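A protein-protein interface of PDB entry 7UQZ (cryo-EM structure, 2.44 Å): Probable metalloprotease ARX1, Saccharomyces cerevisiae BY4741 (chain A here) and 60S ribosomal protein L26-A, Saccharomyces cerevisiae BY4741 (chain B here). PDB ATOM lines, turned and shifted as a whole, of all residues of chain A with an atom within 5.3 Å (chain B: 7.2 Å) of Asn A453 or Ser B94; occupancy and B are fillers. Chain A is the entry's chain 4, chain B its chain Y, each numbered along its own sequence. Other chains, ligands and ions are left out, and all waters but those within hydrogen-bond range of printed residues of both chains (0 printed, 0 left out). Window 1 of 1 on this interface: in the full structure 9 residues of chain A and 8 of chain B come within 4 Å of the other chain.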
ATOM      1  N   ALA A 451      17.556 -14.848 -17.291  1.00  0.00           N
ATOM      2  CA  ALA A 451      18.112 -15.620 -16.192  1.00  0.00           C
ATOM      3  C   ALA A 451      17.385 -15.323 -14.883  1.00  0.00           C
ATOM      4  O   ALA A 451      16.779 -14.264 -14.697  1.00  0.00           O
ATOM      5  CB  ALA A 451      19.598 -15.320 -16.033  1.00  0.00           C
ATOM      6  N   THR A 452      17.454 -16.285 -13.965  1.00  0.00           N
ATOM      7  CA  THR A 452      16.876 -16.164 -12.634  1.00  0.00           C
ATOM      8  C   THR A 452      17.964 -16.376 -11.592  1.00  0.00           C
ATOM      9  O   THR A 452      18.779 -17.296 -11.719  1.00  0.00           O
ATOM     10  CB  THR A 452      15.750 -17.179 -12.422  1.00  0.00           C
ATOM     11  OG1 THR A 452      16.264 -18.506 -12.589  1.00  0.00           O
ATOM     12  CG2 THR A 452      14.624 -16.947 -13.415  1.00  0.00           C
ATOM     13  N   ASN A 453      17.980 -15.525 -10.573  1.00  0.00           N
ATOM     14  CA  ASN A 453      18.901 -15.662  -9.445  1.00  0.00           C
ATOM     15  C   ASN A 453      18.108 -15.580  -8.148  1.00  0.00           C
ATOM     16  O   ASN A 453      17.645 -14.482  -7.777  1.00  0.00           O
ATOM     17  CB  ASN A 453      19.996 -14.598  -9.491  1.00  0.00           C
ATOM     18  CG  ASN A 453      19.474 -13.241  -9.901  1.00  0.00           C
ATOM     19  OD1 ASN A 453      18.483 -13.137 -10.622  1.00  0.00           O
ATOM     20  ND2 ASN A 453      20.140 -12.190  -9.442  1.00  0.00           N
ATOM     21  N   PRO A 454      17.917 -16.698  -7.439  1.00  0.00           N
ATOM     22  CA  PRO A 454      17.096 -16.664  -6.217  1.00  0.00           C
ATOM     23  C   PRO A 454      17.704 -15.864  -5.076  1.00  0.00           C
ATOM     24  O   PRO A 454      16.981 -15.530  -4.130  1.00  0.00           O
ATOM     25  CB  PRO A 454      16.960 -18.148  -5.843  1.00  0.00           C
ATOM     26  CG  PRO A 454      17.252 -18.892  -7.109  1.00  0.00           C
ATOM     27  CD  PRO A 454      18.280 -18.071  -7.822  1.00  0.00           C
ATOM     28  N   ASN A 455      18.997 -15.551  -5.123  1.00  0.00           N
ATOM     29  CA  ASN A 455      19.653 -14.813  -4.049  1.00  0.00           C
ATOM     30  C   ASN A 455      19.741 -13.317  -4.311  1.00  0.00           C
ATOM     31  O   ASN A 455      19.616 -12.524  -3.373  1.00  0.00           O
ATOM     32  CB  ASN A 455      21.060 -15.369  -3.809  1.00  0.00           C
ATOM     33  CG  ASN A 455      21.044 -16.799  -3.311  1.00  0.00           C
ATOM     34  OD1 ASN A 455      20.158 -17.195  -2.555  1.00  0.00           O
ATOM     35  ND2 ASN A 455      22.028 -17.583  -3.734  1.00  0.00           N
ATOM     36  N   GLY A 456      19.954 -12.908  -5.559  1.00  0.00           N
ATOM     37  CA  GLY A 456      20.032 -11.497  -5.886  1.00  0.00           C
ATOM     38  C   GLY A 456      21.287 -10.816  -5.380  1.00  0.00           C
ATOM     39  O   GLY A 456      22.401 -11.231  -5.706  1.00  0.00           O
ATOM     40  N   LEU A 478      20.314  -4.638 -11.535  1.00  0.00           N
ATOM     41  CA  LEU A 478      19.665  -5.927 -11.726  1.00  0.00           C
ATOM     42  C   LEU A 478      19.901  -6.892 -10.574  1.00  0.00           C
ATOM     43  O   LEU A 478      19.271  -7.955 -10.539  1.00  0.00           O
ATOM     44  CB  LEU A 478      20.140  -6.573 -13.030  1.00  0.00           C
ATOM     45  CG  LEU A 478      19.595  -5.965 -14.320  1.00  0.00           C
ATOM     46  CD1 LEU A 478      20.228  -6.633 -15.524  1.00  0.00           C
ATOM     47  CD2 LEU A 478      18.084  -6.093 -14.366  1.00  0.00           C
ATOM     48  N   GLY A 479      20.777  -6.551  -9.636  1.00  0.00           N
ATOM     49  CA  GLY A 479      21.085  -7.439  -8.528  1.00  0.00           C
ATOM     50  C   GLY A 479      21.757  -8.734  -8.931  1.00  0.00           C
ATOM     51  O   GLY A 479      21.432  -9.792  -8.379  1.00  0.00           O
ATOM     52  N   VAL A 480      22.690  -8.679  -9.877  1.00  0.00           N
ATOM     53  CA  VAL A 480      23.416  -9.852 -10.350  1.00  0.00           C
ATOM     54  C   VAL A 480      24.860  -9.726  -9.887  1.00  0.00           C
ATOM     55  O   VAL A 480      25.540  -8.746 -10.214  1.00  0.00           O
ATOM     56  CB  VAL A 480      23.333  -9.992 -11.878  1.00  0.00           C
ATOM     57  CG1 VAL A 480      24.073 -11.239 -12.340  1.00  0.00           C
ATOM     58  CG2 VAL A 480      21.881 -10.027 -12.329  1.00  0.00           C
ATOM     59  N   LYS A 484      27.151 -15.097 -10.121  1.00  0.00           N
ATOM     60  CA  LYS A 484      26.013 -15.291 -11.013  1.00  0.00           C
ATOM     61  C   LYS A 484      26.360 -14.913 -12.448  1.00  0.00           C
ATOM     62  O   LYS A 484      25.945 -15.595 -13.391  1.00  0.00           O
ATOM     63  CB  LYS A 484      24.816 -14.481 -10.520  1.00  0.00           C
ATOM     64  CG  LYS A 484      23.522 -14.807 -11.242  1.00  0.00           C
ATOM     65  CD  LYS A 484      23.228 -16.293 -11.166  1.00  0.00           C
ATOM     66  CE  LYS A 484      22.080 -16.681 -12.075  1.00  0.00           C
ATOM     67  NZ  LYS A 484      21.854 -18.151 -12.052  1.00  0.00           N
ATOM     68  N   THR B  86       7.976 -15.547 -13.153  1.00  0.00           N
ATOM     69  CA  THR B  86       8.819 -15.553 -11.965  1.00  0.00           C
ATOM     70  C   THR B  86       8.183 -14.707 -10.870  1.00  0.00           C
ATOM     71  O   THR B  86       7.199 -13.996 -11.087  1.00  0.00           O
ATOM     72  CB  THR B  86      10.235 -15.026 -12.257  1.00  0.00           C
ATOM     73  OG1 THR B  86      10.152 -13.774 -12.947  1.00  0.00           O
ATOM     74  CG2 THR B  86      11.032 -16.016 -13.093  1.00  0.00           C
ATOM     75  N   LYS B  87       8.768 -14.801  -9.680  1.00  0.00           N
ATOM     76  CA  LYS B  87       8.433 -13.959  -8.541  1.00  0.00           C
ATOM     77  C   LYS B  87       9.656 -13.126  -8.193  1.00  0.00           C
ATOM     78  O   LYS B  87      10.762 -13.665  -8.078  1.00  0.00           O
ATOM     79  CB  LYS B  87       7.995 -14.802  -7.340  1.00  0.00           C
ATOM     80  CG  LYS B  87       7.638 -13.996  -6.102  1.00  0.00           C
ATOM     81  CD  LYS B  87       7.101 -14.896  -5.002  1.00  0.00           C
ATOM     82  CE  LYS B  87       6.561 -14.089  -3.831  1.00  0.00           C
ATOM     83  NZ  LYS B  87       7.617 -13.274  -3.175  1.00  0.00           N
ATOM     84  N   GLU B  88       9.463 -11.823  -8.029  1.00  0.00           N
ATOM     85  CA  GLU B  88      10.561 -10.888  -7.842  1.00  0.00           C
ATOM     86  C   GLU B  88      10.567 -10.351  -6.419  1.00  0.00           C
ATOM     87  O   GLU B  88       9.511 -10.099  -5.832  1.00  0.00           O
ATOM     88  CB  GLU B  88      10.470  -9.721  -8.830  1.00  0.00           C
ATOM     89  CG  GLU B  88      10.796 -10.086 -10.269  1.00  0.00           C
ATOM     90  CD  GLU B  88       9.668 -10.821 -10.962  1.00  0.00           C
ATOM     91  OE1 GLU B  88       8.523 -10.753 -10.471  1.00  0.00           O
ATOM     92  OE2 GLU B  88       9.930 -11.469 -11.998  1.00  0.00           O
ATOM     93  N   LYS B  89      11.765 -10.178  -5.872  1.00  0.00           N
ATOM     94  CA  LYS B  89      11.964  -9.590  -4.559  1.00  0.00           C
ATOM     95  C   LYS B  89      12.551  -8.191  -4.705  1.00  0.00           C
ATOM     96  O   LYS B  89      12.905  -7.749  -5.801  1.00  0.00           O
ATOM     97  CB  LYS B  89      12.879 -10.470  -3.699  1.00  0.00           C
ATOM     98  CG  LYS B  89      12.430 -11.917  -3.597  1.00  0.00           C
ATOM     99  CD  LYS B  89      13.373 -12.730  -2.728  1.00  0.00           C
ATOM    100  CE  LYS B  89      12.987 -14.197  -2.723  1.00  0.00           C
ATOM    101  NZ  LYS B  89      13.915 -15.014  -1.896  1.00  0.00           N
ATOM    102  N   ASN B  91      15.384  -7.114  -3.440  1.00  0.00           N
ATOM    103  CA  ASN B  91      16.830  -7.168  -3.622  1.00  0.00           C
ATOM    104  C   ASN B  91      17.250  -7.704  -4.991  1.00  0.00           C
ATOM    105  O   ASN B  91      18.406  -8.114  -5.149  1.00  0.00           O
ATOM    106  CB  ASN B  91      17.475  -8.007  -2.513  1.00  0.00           C
ATOM    107  CG  ASN B  91      16.844  -9.382  -2.364  1.00  0.00           C
ATOM    108  OD1 ASN B  91      16.127  -9.855  -3.245  1.00  0.00           O
ATOM    109  ND2 ASN B  91      17.113 -10.032  -1.240  1.00  0.00           N
ATOM    110  N   GLY B  92      16.354  -7.717  -5.975  1.00  0.00           N
ATOM    111  CA  GLY B  92      16.691  -8.167  -7.306  1.00  0.00           C
ATOM    112  C   GLY B  92      16.598  -9.659  -7.533  1.00  0.00           C
ATOM    113  O   GLY B  92      16.910 -10.120  -8.637  1.00  0.00           O
ATOM    114  N   ALA B  93      16.180 -10.428  -6.532  1.00  0.00           N
ATOM    115  CA  ALA B  93      16.094 -11.872  -6.670  1.00  0.00           C
ATOM    116  C   ALA B  93      14.862 -12.270  -7.474  1.00  0.00           C
ATOM    117  O   ALA B  93      13.782 -11.696  -7.308  1.00  0.00           O
ATOM    118  CB  ALA B  93      16.061 -12.538  -5.297  1.00  0.00           C
ATOM    119  N   SER B  94      15.032 -13.258  -8.350  1.00  0.00           N
ATOM    120  CA  SER B  94      13.942 -13.795  -9.159  1.00  0.00           C
ATOM    121  C   SER B  94      13.865 -15.297  -8.935  1.00  0.00           C
ATOM    122  O   SER B  94      14.858 -16.006  -9.122  1.00  0.00           O
ATOM    123  CB  SER B  94      14.142 -13.483 -10.643  1.00  0.00           C
ATOM    124  OG  SER B  94      14.100 -12.088 -10.882  1.00  0.00           O
ATOM    125  N   VAL B  95      12.694 -15.775  -8.544  1.00  0.00           N
ATOM    126  CA  VAL B  95      12.460 -17.183  -8.237  1.00  0.00           C
ATOM    127  C   VAL B  95      11.487 -17.735  -9.271  1.00  0.00           C
ATOM    128  O   VAL B  95      10.429 -17.136  -9.485  1.00  0.00           O
ATOM    129  CB  VAL B  95      11.900 -17.372  -6.814  1.00  0.00           C
ATOM    130  CG1 VAL B  95      11.841 -18.846  -6.462  1.00  0.00           C
ATOM    131  CG2 VAL B  95      12.742 -16.612  -5.809  1.00  0.00           C
ATOM    132  N   PRO B  96      11.808 -18.839  -9.941  1.00  0.00           N
ATOM    133  CA  PRO B  96      10.861 -19.418 -10.904  1.00  0.00           C
ATOM    134  C   PRO B  96       9.577 -19.880 -10.228  1.00  0.00           C
ATOM    135  O   PRO B  96       9.586 -20.364  -9.095  1.00  0.00           O
ATOM    136  CB  PRO B  96      11.637 -20.599 -11.498  1.00  0.00           C
ATOM    137  CG  PRO B  96      13.074 -20.281 -11.248  1.00  0.00           C
ATOM    138  CD  PRO B  96      13.108 -19.531  -9.954  1.00  0.00           C
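N of Ser B94 is in hydrogen-bond range of O of Asn A453 (2.9 Å).
The side-chain hydroxyl (OG1) of Thr B86 lies within hydrogen-bond range of the side-chain carboxylate (OE2) of Glu B88 (2.5 Å).
N of Ala B93 sits close to OD1 of Asn B91.
O of Thr A452 sits at hydrogen-bond distance from NZ of Lys A484.
The backbone carbonyl oxygen (O) of Gly A479 is in hydrogen-bond range of the side-chain amide nitrogen (ND2) of Asn A453 (2.9 Å).
Among the printed residues, pairs that only touch across the chains: Asn A453 with Ala B93, Pro A454 with Ala B93, Pro A454 with Ser B94, Thr A452 with Ser B94, Thr A452 with Thr B86, Leu A478 with Gly B92, Gly A456 with Asn B91, Pro A454 with Lys B89, Asn A455 with Ala B93, Thr A452 with Pro B96, Gly A456 with Ala B93 and Asn A453 with Gly B92.
Of the printed residues of chain B, Asn A453 touches Gly B92 (3.9 Å), Ala B93 (3.2 Å) and Ser B94 (2.9 Å).
Ser B94 touches just these residues of chain A: Thr A452 (3.6 Å), Asn A453 (2.9 Å) and Pro A454 (3.6 Å).
Printed residues of chain A within 4 Å of Gly B92: Asn A453 and Leu A478.
Of the printed residues of chain B, Pro A454 touches Lys B89 (3.8 Å), Ala B93 (3.3 Å) and Ser B94 (3.6 Å).
Of the printed residues of chain A, Pro B96 touches Thr A452.
Of the printed residues of chain A, Lys B89 touches Pro A454 (3.8 Å).
Ala A451 touches none of the printed residues of chain B.
The nearest residue of chain A that does not touch Ser B94 is Ala A451 (4.9 Å).
The nearest printed residue of chain B that does not touch Gly A456 is Gly B92 (4.2 Å).
Printed residues of chain A that touch a printed residue of chain B: Thr A452, Asn A453, Pro A454, Asn A455, Gly A456 and Leu A478.
Of the 10 printed residues of chain B, 7 touch a printed residue of chain A.
Along chain B the printed residues that touch a printed residue of chain A span positions 86 to 96.
Among the printed residues, 13 pairs touch across the chains.
Among the printed residues, no Asp or Glu carboxylate lies within 4 Å of a Lys or Arg side-chain nitrogen of the other chain.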
